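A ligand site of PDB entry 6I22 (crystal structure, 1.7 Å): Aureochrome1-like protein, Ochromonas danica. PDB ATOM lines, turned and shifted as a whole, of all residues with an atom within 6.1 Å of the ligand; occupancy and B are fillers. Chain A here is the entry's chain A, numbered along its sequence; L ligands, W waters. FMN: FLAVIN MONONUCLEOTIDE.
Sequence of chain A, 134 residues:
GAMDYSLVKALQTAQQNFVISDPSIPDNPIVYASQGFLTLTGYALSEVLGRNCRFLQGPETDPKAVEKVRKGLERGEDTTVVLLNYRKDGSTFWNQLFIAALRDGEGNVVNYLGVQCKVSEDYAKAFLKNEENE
Water W1 bridges OE1 of Gln 57 (2.6 Å) and O1P of the ligand (2.7 Å). Water W5 lies within hydrogen-bond range of the side-chain carboxylate of Glu 67 and an oxygen (O2P) of the ligand. Water W2 lies within hydrogen-bond range of an oxygen (O3') of the ligand (3.0 Å), the side-chain amide nitrogen of Asn 28 (3.2 Å) and the side-chain amide nitrogen of Asn 52 (3.2 Å). Water W6 lies within hydrogen-bond range of the backbone carbonyl oxygen of Asn 28 (3.0 Å), the backbone NH of Cys 53 (3.1 Å) and an oxygen (O2') of the ligand (3.2 Å).
Val 19 touches the ligand (CG2 to C6, 3.5 Å). Ser 21 touches the ligand (OG to C8M, 3.9 Å). Asn 28 touches the ligand. Leu 56 touches the ligand (CD1 to O4, 3.5 Å). Val 66 touches the ligand. Val 69 touches the ligand (CG1 to C1', 3.9 Å). CD of Arg 70 touches O2P of the ligand, 3.5 Å away. Leu 73 touches the ligand (CD2 to O3', 3.8 Å). Leu 83 touches the ligand. Leu 97 touches the ligand (CD1 to N5, 3.5 Å). Ile 99 touches the ligand (CD1 to C9, 3.7 Å). CB of Tyr 112 touches C7M of the ligand, 3.8 Å away. C of Leu 113 touches C7M of the ligand, 3.8 Å away. N of Gly 114 touches C7M of the ligand, at 3.5 Å. Of the 29 residues printed, 21 come within 4 Å of the ligand. Along chain A the residues within 4 Å of the ligand span positions 19 to 116. The nearest printed residue that does not touch the ligand is Phe 37 (4.4 Å).
OD1 of Asn 52 lies within hydrogen-bond range of O2' of the ligand. A nitrogen (N5) of the ligand is in hydrogen-bond range of the side-chain sulfur of Cys 53 (3.4 Å). NE2 of Gln 57 sits at hydrogen-bond distance from O2 of the ligand, at 2.9 Å. The side-chain amide nitrogen (NE2) of Gln 116 lies within hydrogen-bond range of an oxygen (O4) of the ligand (3.1 Å). The side-chain amide nitrogen (ND2) of Asn 95 is in hydrogen-bond range of an oxygen (O4) of the ligand (3.1 Å). The side-chain amide nitrogen of Asn 85 sits close to a nitrogen (N3) of the ligand (2.9 Å). O3P of the ligand lies within salt-bridge range of NH2 of Arg 54 (2.8 Å).
The side-chain amide nitrogen (ND2) of Asn 85 lies close to the side-chain amide nitrogen (ND2) of Asn 95, at 2.8 Å. N of Asn 95 sits at hydrogen-bond distance from O of Leu 83. The guanidinium group (NH1) of Arg 70 lies within salt-bridge range of the side-chain carboxylate (OE2) of Glu 67 (3.1 Å). The backbone carbonyl oxygen of Tyr 112 lies within hydrogen-bond range of the backbone NH of Ser 21 (2.9 Å). The side-chain amide oxygen (OD1) of Asn 28 sits at hydrogen-bond distance from the side-chain hydroxyl (OG) of Ser 21, 2.7 Å away. ND2 of Asn 52 lies within hydrogen-bond range of O of Asp 27, at 2.8 Å. OD1 of Asn 52 is in hydrogen-bond range of N of Arg 54 (2.9 Å). The side-chain carboxylate (OD2) of Asp 27 lies within salt-bridge range of the guanidinium group (NH1) of Arg 54 (3.0 Å).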
ATOM      1  N   VAL A  19      15.304 -33.855   7.559  1.00  0.00           N
ATOM      2  CA  VAL A  19      15.278 -33.945   9.038  1.00  0.00           C
ATOM      3  C   VAL A  19      13.908 -33.494   9.513  1.00  0.00           C
ATOM      4  O   VAL A  19      13.192 -32.780   8.804  1.00  0.00           O
ATOM      5  CB  VAL A  19      16.387 -33.115   9.677  1.00  0.00           C
ATOM      6  CG1 VAL A  19      17.776 -33.511   9.159  1.00  0.00           C
ATOM      7  CG2 VAL A  19      16.133 -31.633   9.483  1.00  0.00           C
ATOM      8  N   ILE A  20      13.564 -34.021  10.672  1.00  0.00           N
ATOM      9  CA  ILE A  20      12.368 -33.616  11.437  1.00  0.00           C
ATOM     10  C   ILE A  20      12.836 -32.999  12.755  1.00  0.00           C
ATOM     11  O   ILE A  20      13.678 -33.621  13.436  1.00  0.00           O
ATOM     12  CB  ILE A  20      11.464 -34.825  11.645  1.00  0.00           C
ATOM     13  CG1 ILE A  20      10.987 -35.403  10.312  1.00  0.00           C
ATOM     14  CG2 ILE A  20      10.300 -34.493  12.546  1.00  0.00           C
ATOM     15  CD1 ILE A  20      10.353 -36.737  10.498  1.00  0.00           C
ATOM     16  N   SER A  21      12.309 -31.832  13.097  1.00  0.00           N
ATOM     17  CA  SER A  21      12.614 -31.140  14.351  1.00  0.00           C
ATOM     18  C   SER A  21      11.389 -31.167  15.254  1.00  0.00           C
ATOM     19  O   SER A  21      10.220 -31.311  14.735  1.00  0.00           O
ATOM     20  CB  SER A  21      13.094 -29.738  14.106  1.00  0.00           C
ATOM     21  OG  SER A  21      11.998 -28.871  13.895  1.00  0.00           O
ATOM     22  N   ASP A  27      15.157 -25.172  21.852  1.00  0.00           N
ATOM     23  CA  ASP A  27      16.004 -24.885  20.665  1.00  0.00           C
ATOM     24  C   ASP A  27      15.619 -25.715  19.426  1.00  0.00           C
ATOM     25  O   ASP A  27      16.425 -25.797  18.481  1.00  0.00           O
ATOM     26  CB  ASP A  27      17.498 -25.017  20.975  1.00  0.00           C
ATOM     27  CG  ASP A  27      18.380 -24.203  20.045  1.00  0.00           C
ATOM     28  OD1 ASP A  27      17.940 -23.152  19.538  1.00  0.00           O
ATOM     29  OD2 ASP A  27      19.493 -24.659  19.786  1.00  0.00           O
ATOM     30  N   ASN A  28      14.442 -26.347  19.409  1.00  0.00           N
ATOM     31  CA  ASN A  28      13.853 -26.980  18.188  1.00  0.00           C
ATOM     32  C   ASN A  28      14.845 -27.927  17.534  1.00  0.00           C
ATOM     33  O   ASN A  28      15.217 -27.781  16.363  1.00  0.00           O
ATOM     34  CB  ASN A  28      13.443 -25.910  17.183  1.00  0.00           C
ATOM     35  CG  ASN A  28      12.617 -26.465  16.037  1.00  0.00           C
ATOM     36  OD1 ASN A  28      11.884 -27.460  16.180  1.00  0.00           O
ATOM     37  ND2 ASN A  28      12.722 -25.793  14.892  1.00  0.00           N
ATOM     38  N   PHE A  37      20.524 -37.457   4.472  1.00  0.00           N
ATOM     39  CA  PHE A  37      21.067 -36.281   5.199  1.00  0.00           C
ATOM     40  C   PHE A  37      22.402 -36.663   5.862  1.00  0.00           C
ATOM     41  O   PHE A  37      23.359 -35.874   5.792  1.00  0.00           O
ATOM     42  CB  PHE A  37      20.064 -35.784   6.238  1.00  0.00           C
ATOM     43  CG  PHE A  37      20.590 -34.680   7.122  1.00  0.00           C
ATOM     44  CD1 PHE A  37      20.470 -33.363   6.736  1.00  0.00           C
ATOM     45  CD2 PHE A  37      21.213 -34.961   8.334  1.00  0.00           C
ATOM     46  CE1 PHE A  37      20.958 -32.335   7.533  1.00  0.00           C
ATOM     47  CE2 PHE A  37      21.700 -33.940   9.122  1.00  0.00           C
ATOM     48  CZ  PHE A  37      21.568 -32.636   8.736  1.00  0.00           C
ATOM     49  N   ASN A  52      20.084 -28.478  17.181  1.00  0.00           N
ATOM     50  CA  ASN A  52      19.523 -27.588  16.136  1.00  0.00           C
ATOM     51  C   ASN A  52      20.409 -27.722  14.901  1.00  0.00           C
ATOM     52  O   ASN A  52      21.649 -27.798  15.003  1.00  0.00           O
ATOM     53  CB  ASN A  52      19.440 -26.158  16.628  1.00  0.00           C
ATOM     54  CG  ASN A  52      18.720 -25.242  15.670  1.00  0.00           C
ATOM     55  OD1 ASN A  52      19.299 -24.879  14.639  1.00  0.00           O
ATOM     56  ND2 ASN A  52      17.500 -24.868  16.022  1.00  0.00           N
ATOM     57  N   CYS A  53      19.789 -27.720  13.732  1.00  0.00           N
ATOM     58  CA  CYS A  53      20.458 -27.922  12.423  1.00  0.00           C
ATOM     59  C   CYS A  53      21.429 -26.784  12.068  1.00  0.00           C
ATOM     60  O   CYS A  53      22.184 -26.942  11.088  1.00  0.00           O
ATOM     61  CB  CYS A  53      19.407 -28.087  11.320  1.00  0.00           C
ATOM     62  SG  CYS A  53      19.832 -29.455  10.202  1.00  0.00           S
ATOM     63  N   ARG A  54      21.453 -25.690  12.826  1.00  0.00           N
ATOM     64  CA  ARG A  54      22.407 -24.587  12.524  1.00  0.00           C
ATOM     65  C   ARG A  54      23.871 -25.033  12.644  1.00  0.00           C
ATOM     66  O   ARG A  54      24.722 -24.244  12.204  1.00  0.00           O
ATOM     67  CB  ARG A  54      22.152 -23.341  13.373  1.00  0.00           C
ATOM     68  CG  ARG A  54      22.614 -23.475  14.820  1.00  0.00           C
ATOM     69  CD  ARG A  54      22.480 -22.159  15.544  1.00  0.00           C
ATOM     70  NE  ARG A  54      21.096 -21.793  15.719  1.00  0.00           N
ATOM     71  CZ  ARG A  54      20.300 -22.240  16.689  1.00  0.00           C
ATOM     72  NH1 ARG A  54      20.760 -23.073  17.609  1.00  0.00           N
ATOM     73  NH2 ARG A  54      19.057 -21.811  16.729  1.00  0.00           N
ATOM     74  N   LEU A  56      25.366 -26.922  10.808  1.00  0.00           N
ATOM     75  CA  LEU A  56      25.861 -27.021   9.406  1.00  0.00           C
ATOM     76  C   LEU A  56      26.412 -25.687   8.882  1.00  0.00           C
ATOM     77  O   LEU A  56      26.972 -25.668   7.758  1.00  0.00           O
ATOM     78  CB  LEU A  56      24.710 -27.487   8.518  1.00  0.00           C
ATOM     79  CG  LEU A  56      24.261 -28.935   8.717  1.00  0.00           C
ATOM     80  CD1 LEU A  56      23.115 -29.257   7.772  1.00  0.00           C
ATOM     81  CD2 LEU A  56      25.400 -29.907   8.532  1.00  0.00           C
ATOM     82  N   GLN A  57      26.221 -24.581   9.609  1.00  0.00           N
ATOM     83  CA  GLN A  57      26.619 -23.241   9.147  1.00  0.00           C
ATOM     84  C   GLN A  57      28.078 -22.950   9.541  1.00  0.00           C
ATOM     85  O   GLN A  57      28.570 -23.553  10.487  1.00  0.00           O
ATOM     86  CB  GLN A  57      25.607 -22.232   9.683  1.00  0.00           C
ATOM     87  CG  GLN A  57      24.200 -22.476   9.183  1.00  0.00           C
ATOM     88  CD  GLN A  57      23.126 -21.806  10.019  1.00  0.00           C
ATOM     89  OE1 GLN A  57      23.431 -20.918  10.815  1.00  0.00           O
ATOM     90  NE2 GLN A  57      21.871 -22.183   9.776  1.00  0.00           N
ATOM     91  N   THR A  61      28.954 -19.075   5.216  1.00  0.00           N
ATOM     92  CA  THR A  61      27.469 -19.053   5.212  1.00  0.00           C
ATOM     93  C   THR A  61      27.042 -17.588   5.265  1.00  0.00           C
ATOM     94  O   THR A  61      27.600 -16.836   6.076  1.00  0.00           O
ATOM     95  CB  THR A  61      26.879 -19.857   6.370  1.00  0.00           C
ATOM     96  OG1 THR A  61      27.413 -21.186   6.348  1.00  0.00           O
ATOM     97  CG2 THR A  61      25.378 -19.916   6.290  1.00  0.00           C
ATOM     98  N   VAL A  66      20.460 -17.147   6.679  1.00  0.00           N
ATOM     99  CA  VAL A  66      20.098 -17.746   7.994  1.00  0.00           C
ATOM    100  C   VAL A  66      18.937 -16.933   8.603  1.00  0.00           C
ATOM    101  O   VAL A  66      17.995 -17.554   9.087  1.00  0.00           O
ATOM    102  CB  VAL A  66      21.321 -17.818   8.927  1.00  0.00           C
ATOM    103  CG1 VAL A  66      20.937 -18.310  10.318  1.00  0.00           C
ATOM    104  CG2 VAL A  66      22.405 -18.686   8.311  1.00  0.00           C
ATOM    105  N   GLU A  67      19.010 -15.627   8.554  1.00  0.00           N
ATOM    106  CA  GLU A  67      17.970 -14.724   9.098  1.00  0.00           C
ATOM    107  C   GLU A  67      16.627 -14.941   8.365  1.00  0.00           C
ATOM    108  O   GLU A  67      15.564 -14.866   9.035  1.00  0.00           O
ATOM    109  CB  GLU A  67      18.449 -13.283   8.975  1.00  0.00           C
ATOM    110  CG  GLU A  67      17.485 -12.266   9.572  1.00  0.00           C
ATOM    111  CD  GLU A  67      17.235 -12.399  11.062  1.00  0.00           C
ATOM    112  OE1 GLU A  67      17.718 -13.388  11.704  1.00  0.00           O
ATOM    113  OE2 GLU A  67      16.546 -11.515  11.593  1.00  0.00           O
ATOM    114  N   VAL A  69      15.556 -17.715   7.145  1.00  0.00           N
ATOM    115  CA  VAL A  69      14.996 -18.968   7.710  1.00  0.00           C
ATOM    116  C   VAL A  69      14.363 -18.625   9.058  1.00  0.00           C
ATOM    117  O   VAL A  69      13.206 -18.998   9.273  1.00  0.00           O
ATOM    118  CB  VAL A  69      16.040 -20.073   7.818  1.00  0.00           C
ATOM    119  CG1 VAL A  69      15.447 -21.290   8.501  1.00  0.00           C
ATOM    120  CG2 VAL A  69      16.610 -20.423   6.461  1.00  0.00           C
ATOM    121  N   ARG A  70      15.106 -17.944   9.938  1.00  0.00           N
ATOM    122  CA  ARG A  70      14.614 -17.647  11.307  1.00  0.00           C
ATOM    123  C   ARG A  70      13.289 -16.896  11.211  1.00  0.00           C
ATOM    124  O   ARG A  70      12.359 -17.259  11.942  1.00  0.00           O
ATOM    125  CB  ARG A  70      15.621 -16.808  12.095  1.00  0.00           C
ATOM    126  CG  ARG A  70      15.364 -16.805  13.600  1.00  0.00           C
ATOM    127  CD  ARG A  70      16.040 -15.627  14.263  1.00  0.00           C
ATOM    128  NE  ARG A  70      15.148 -14.532  13.921  1.00  0.00           N
ATOM    129  CZ  ARG A  70      15.387 -13.236  14.075  1.00  0.00           C
ATOM    130  NH1 ARG A  70      14.453 -12.370  13.709  1.00  0.00           N
ATOM    131  NH2 ARG A  70      16.535 -12.813  14.567  1.00  0.00           N
ATOM    132  N   LEU A  73      10.192 -19.049   9.947  1.00  0.00           N
ATOM    133  CA  LEU A  73       9.637 -19.968  10.981  1.00  0.00           C
ATOM    134  C   LEU A  73       8.829 -19.140  11.978  1.00  0.00           C
ATOM    135  O   LEU A  73       7.654 -19.497  12.197  1.00  0.00           O
ATOM    136  CB  LEU A  73      10.777 -20.739  11.641  1.00  0.00           C
ATOM    137  CG  LEU A  73      11.259 -22.012  10.921  1.00  0.00           C
ATOM    138  CD1 LEU A  73      10.881 -22.048   9.446  1.00  0.00           C
ATOM    139  CD2 LEU A  73      12.753 -22.165  11.083  1.00  0.00           C
ATOM    140  N   LEU A  83      21.727 -21.749   0.767  1.00  0.00           N
ATOM    141  CA  LEU A  83      22.862 -21.267   1.608  1.00  0.00           C
ATOM    142  C   LEU A  83      23.976 -22.292   1.655  1.00  0.00           C
ATOM    143  O   LEU A  83      23.772 -23.472   1.372  1.00  0.00           O
ATOM    144  CB  LEU A  83      22.397 -20.812   3.005  1.00  0.00           C
ATOM    145  CG  LEU A  83      21.609 -21.731   3.958  1.00  0.00           C
ATOM    146  CD1 LEU A  83      21.630 -23.204   3.647  1.00  0.00           C
ATOM    147  CD2 LEU A  83      21.965 -21.453   5.409  1.00  0.00           C
ATOM    148  N   LEU A  84      25.168 -21.796   1.960  1.00  0.00           N
ATOM    149  CA  LEU A  84      26.380 -22.640   2.032  1.00  0.00           C
ATOM    150  C   LEU A  84      26.363 -23.376   3.359  1.00  0.00           C
ATOM    151  O   LEU A  84      26.165 -22.719   4.419  1.00  0.00           O
ATOM    152  CB  LEU A  84      27.615 -21.772   1.864  1.00  0.00           C
ATOM    153  CG  LEU A  84      28.887 -22.538   1.552  1.00  0.00           C
ATOM    154  CD1 LEU A  84      28.859 -23.071   0.140  1.00  0.00           C
ATOM    155  CD2 LEU A  84      30.088 -21.649   1.665  1.00  0.00           C
ATOM    156  N   ASN A  85      26.572 -24.684   3.319  1.00  0.00           N
ATOM    157  CA  ASN A  85      26.667 -25.495   4.543  1.00  0.00           C
ATOM    158  C   ASN A  85      27.998 -26.269   4.540  1.00  0.00           C
ATOM    159  O   ASN A  85      28.669 -26.343   3.489  1.00  0.00           O
ATOM    160  CB  ASN A  85      25.493 -26.453   4.690  1.00  0.00           C
ATOM    161  CG  ASN A  85      24.245 -25.880   5.328  1.00  0.00           C
ATOM    162  OD1 ASN A  85      24.187 -24.704   5.777  1.00  0.00           O
ATOM    163  ND2 ASN A  85      23.253 -26.723   5.394  1.00  0.00           N
ATOM    164  N   ASN A  95      23.188 -25.752  -0.329  1.00  0.00           N
ATOM    165  CA  ASN A  95      22.010 -26.478   0.200  1.00  0.00           C
ATOM    166  C   ASN A  95      20.796 -25.651  -0.198  1.00  0.00           C
ATOM    167  O   ASN A  95      20.683 -24.480   0.227  1.00  0.00           O
ATOM    168  CB  ASN A  95      22.184 -26.634   1.704  1.00  0.00           C
ATOM    169  CG  ASN A  95      21.046 -27.357   2.388  1.00  0.00           C
ATOM    170  OD1 ASN A  95      20.089 -27.773   1.717  1.00  0.00           O
ATOM    171  ND2 ASN A  95      21.158 -27.509   3.712  1.00  0.00           N
ATOM    172  N   LEU A  97      17.299 -25.501   0.769  1.00  0.00           N
ATOM    173  CA  LEU A  97      16.633 -25.962   1.988  1.00  0.00           C
ATOM    174  C   LEU A  97      15.157 -25.591   1.901  1.00  0.00           C
ATOM    175  O   LEU A  97      14.857 -24.440   1.646  1.00  0.00           O
ATOM    176  CB  LEU A  97      17.333 -25.254   3.158  1.00  0.00           C
ATOM    177  CG  LEU A  97      16.719 -25.462   4.533  1.00  0.00           C
ATOM    178  CD1 LEU A  97      16.722 -26.944   4.900  1.00  0.00           C
ATOM    179  CD2 LEU A  97      17.511 -24.641   5.552  1.00  0.00           C
ATOM    180  N   ILE A  99      11.638 -25.881   4.041  1.00  0.00           N
ATOM    181  CA  ILE A  99      11.139 -26.151   5.415  1.00  0.00           C
ATOM    182  C   ILE A  99       9.629 -25.917   5.397  1.00  0.00           C
ATOM    183  O   ILE A  99       9.162 -24.875   4.927  1.00  0.00           O
ATOM    184  CB  ILE A  99      11.828 -25.258   6.450  1.00  0.00           C
ATOM    185  CG1 ILE A  99      13.329 -25.534   6.513  1.00  0.00           C
ATOM    186  CG2 ILE A  99      11.172 -25.436   7.798  1.00  0.00           C
ATOM    187  CD1 ILE A  99      14.098 -24.496   7.287  1.00  0.00           C
ATOM    188  N   ALA A 100       8.905 -26.869   5.984  1.00  0.00           N
ATOM    189  CA  ALA A 100       7.466 -26.763   6.212  1.00  0.00           C
ATOM    190  C   ALA A 100       7.129 -27.139   7.659  1.00  0.00           C
ATOM    191  O   ALA A 100       7.741 -28.036   8.222  1.00  0.00           O
ATOM    192  CB  ALA A 100       6.716 -27.629   5.232  1.00  0.00           C
ATOM    193  N   TYR A 112       8.630 -29.617  12.520  1.00  0.00           N
ATOM    194  CA  TYR A 112       9.106 -29.028  11.241  1.00  0.00           C
ATOM    195  C   TYR A 112       9.796 -30.109  10.441  1.00  0.00           C
ATOM    196  O   TYR A 112      10.458 -31.003  10.992  1.00  0.00           O
ATOM    197  CB  TYR A 112      10.058 -27.853  11.441  1.00  0.00           C
ATOM    198  CG  TYR A 112       9.372 -26.647  12.022  1.00  0.00           C
ATOM    199  CD1 TYR A 112       8.719 -25.738  11.207  1.00  0.00           C
ATOM    200  CD2 TYR A 112       9.418 -26.409  13.371  1.00  0.00           C
ATOM    201  CE1 TYR A 112       8.092 -24.635  11.765  1.00  0.00           C
ATOM    202  CE2 TYR A 112       8.811 -25.315  13.933  1.00  0.00           C
ATOM    203  CZ  TYR A 112       8.168 -24.415  13.123  1.00  0.00           C
ATOM    204  OH  TYR A 112       7.533 -23.386  13.750  1.00  0.00           O
ATOM    205  N   LEU A 113       9.580 -30.028   9.139  1.00  0.00           N
ATOM    206  CA  LEU A 113      10.204 -30.944   8.178  1.00  0.00           C
ATOM    207  C   LEU A 113      11.098 -30.083   7.313  1.00  0.00           C
ATOM    208  O   LEU A 113      10.616 -29.085   6.752  1.00  0.00           O
ATOM    209  CB  LEU A 113       9.085 -31.633   7.374  1.00  0.00           C
ATOM    210  CG  LEU A 113       9.555 -32.479   6.190  1.00  0.00           C
ATOM    211  CD1 LEU A 113      10.443 -33.638   6.630  1.00  0.00           C
ATOM    212  CD2 LEU A 113       8.344 -33.079   5.475  1.00  0.00           C
ATOM    213  N   GLY A 114      12.336 -30.508   7.144  1.00  0.00           N
ATOM    214  CA  GLY A 114      13.304 -29.790   6.320  1.00  0.00           C
ATOM    215  C   GLY A 114      13.900 -30.733   5.322  1.00  0.00           C
ATOM    216  O   GLY A 114      14.430 -31.788   5.739  1.00  0.00           O
ATOM    217  N   VAL A 115      13.855 -30.368   4.067  1.00  0.00           N
ATOM    218  CA  VAL A 115      14.450 -31.166   2.962  1.00  0.00           C
ATOM    219  C   VAL A 115      15.652 -30.400   2.436  1.00  0.00           C
ATOM    220  O   VAL A 115      15.487 -29.232   2.118  1.00  0.00           O
ATOM    221  CB  VAL A 115      13.401 -31.439   1.862  1.00  0.00           C
ATOM    222  CG1 VAL A 115      14.020 -32.225   0.706  1.00  0.00           C
ATOM    223  CG2 VAL A 115      12.188 -32.143   2.421  1.00  0.00           C
ATOM    224  N   GLN A 116      16.793 -31.079   2.311  1.00  0.00           N
ATOM    225  CA  GLN A 116      18.045 -30.489   1.817  1.00  0.00           C
ATOM    226  C   GLN A 116      18.321 -31.049   0.432  1.00  0.00           C
ATOM    227  O   GLN A 116      18.404 -32.272   0.289  1.00  0.00           O
ATOM    228  CB  GLN A 116      19.214 -30.835   2.748  1.00  0.00           C
ATOM    229  CG  GLN A 116      19.081 -30.247   4.136  1.00  0.00           C
ATOM    230  CD  GLN A 116      18.255 -31.049   5.097  1.00  0.00           C
ATOM    231  OE1 GLN A 116      17.934 -32.224   4.856  1.00  0.00           O
ATOM    232  NE2 GLN A 116      18.034 -30.463   6.264  1.00  0.00           N
HETATM  233  N1  FMN L   1      19.938 -24.672   8.582  1.00  0.00           N
HETATM  234  C2  FMN L   1      20.963 -24.989   7.770  1.00  0.00           C
HETATM  235  O2  FMN L   1      21.920 -24.175   7.682  1.00  0.00           O
HETATM  236  N3  FMN L   1      20.985 -26.151   7.104  1.00  0.00           N
HETATM  237  C4  FMN L   1      19.994 -27.070   7.150  1.00  0.00           C
HETATM  238  O4  FMN L   1      20.040 -28.140   6.525  1.00  0.00           O
HETATM  239  C4A FMN L   1      18.830 -26.796   8.007  1.00  0.00           C
HETATM  240  N5  FMN L   1      17.783 -27.656   8.134  1.00  0.00           N
HETATM  241  C5A FMN L   1      16.737 -27.305   8.924  1.00  0.00           C
HETATM  242  C6  FMN L   1      15.664 -28.167   9.082  1.00  0.00           C
HETATM  243  C7  FMN L   1      14.589 -27.854   9.906  1.00  0.00           C
HETATM  244  C7M FMN L   1      13.428 -28.835  10.005  1.00  0.00           C
HETATM  245  C8  FMN L   1      14.599 -26.559  10.582  1.00  0.00           C
HETATM  246  C8M FMN L   1      13.460 -26.165  11.483  1.00  0.00           C
HETATM  247  C9  FMN L   1      15.669 -25.689  10.468  1.00  0.00           C
HETATM  248  C9A FMN L   1      16.742 -26.016   9.643  1.00  0.00           C
HETATM  249  N10 FMN L   1      17.832 -25.140   9.521  1.00  0.00           N
HETATM  250  C10 FMN L   1      18.892 -25.502   8.698  1.00  0.00           C
HETATM  251  C1' FMN L   1      17.886 -23.819  10.131  1.00  0.00           C
HETATM  252  C2' FMN L   1      18.351 -23.688  11.583  1.00  0.00           C
HETATM  253  O2' FMN L   1      17.840 -24.751  12.338  1.00  0.00           O
HETATM  254  C3' FMN L   1      17.848 -22.375  12.189  1.00  0.00           C
HETATM  255  O3' FMN L   1      16.413 -22.365  12.185  1.00  0.00           O
HETATM  256  C4' FMN L   1      18.399 -21.171  11.423  1.00  0.00           C
HETATM  257  O4' FMN L   1      19.810 -21.183  11.559  1.00  0.00           O
HETATM  258  C5' FMN L   1      17.846 -19.823  11.925  1.00  0.00           C
HETATM  259  O5' FMN L   1      17.817 -19.770  13.362  1.00  0.00           O
HETATM  260  P   FMN L   1      19.041 -19.059  14.193  1.00  0.00           P
HETATM  261  O1P FMN L   1      20.356 -19.724  13.748  1.00  0.00           O
HETATM  262  O2P FMN L   1      18.942 -17.591  13.792  1.00  0.00           O
HETATM  263  O3P FMN L   1      18.654 -19.314  15.636  1.00  0.00           O
HETATM  264  O   HOH W   1      22.825 -19.310  12.832  1.00  0.00           O
HETATM  265  O   HOH W   2      14.980 -23.529  14.532  1.00  0.00           O
HETATM  266  O   HOH W   3      15.070 -20.527  14.220  1.00  0.00           O
HETATM  267  O   HOH W   4      20.009 -18.447  17.823  1.00  0.00           O
HETATM  268  O   HOH W   5      19.378 -15.474  12.057  1.00  0.00           O
HETATM  269  O   HOH W   6      16.742 -27.437  13.763  1.00  0.00           O
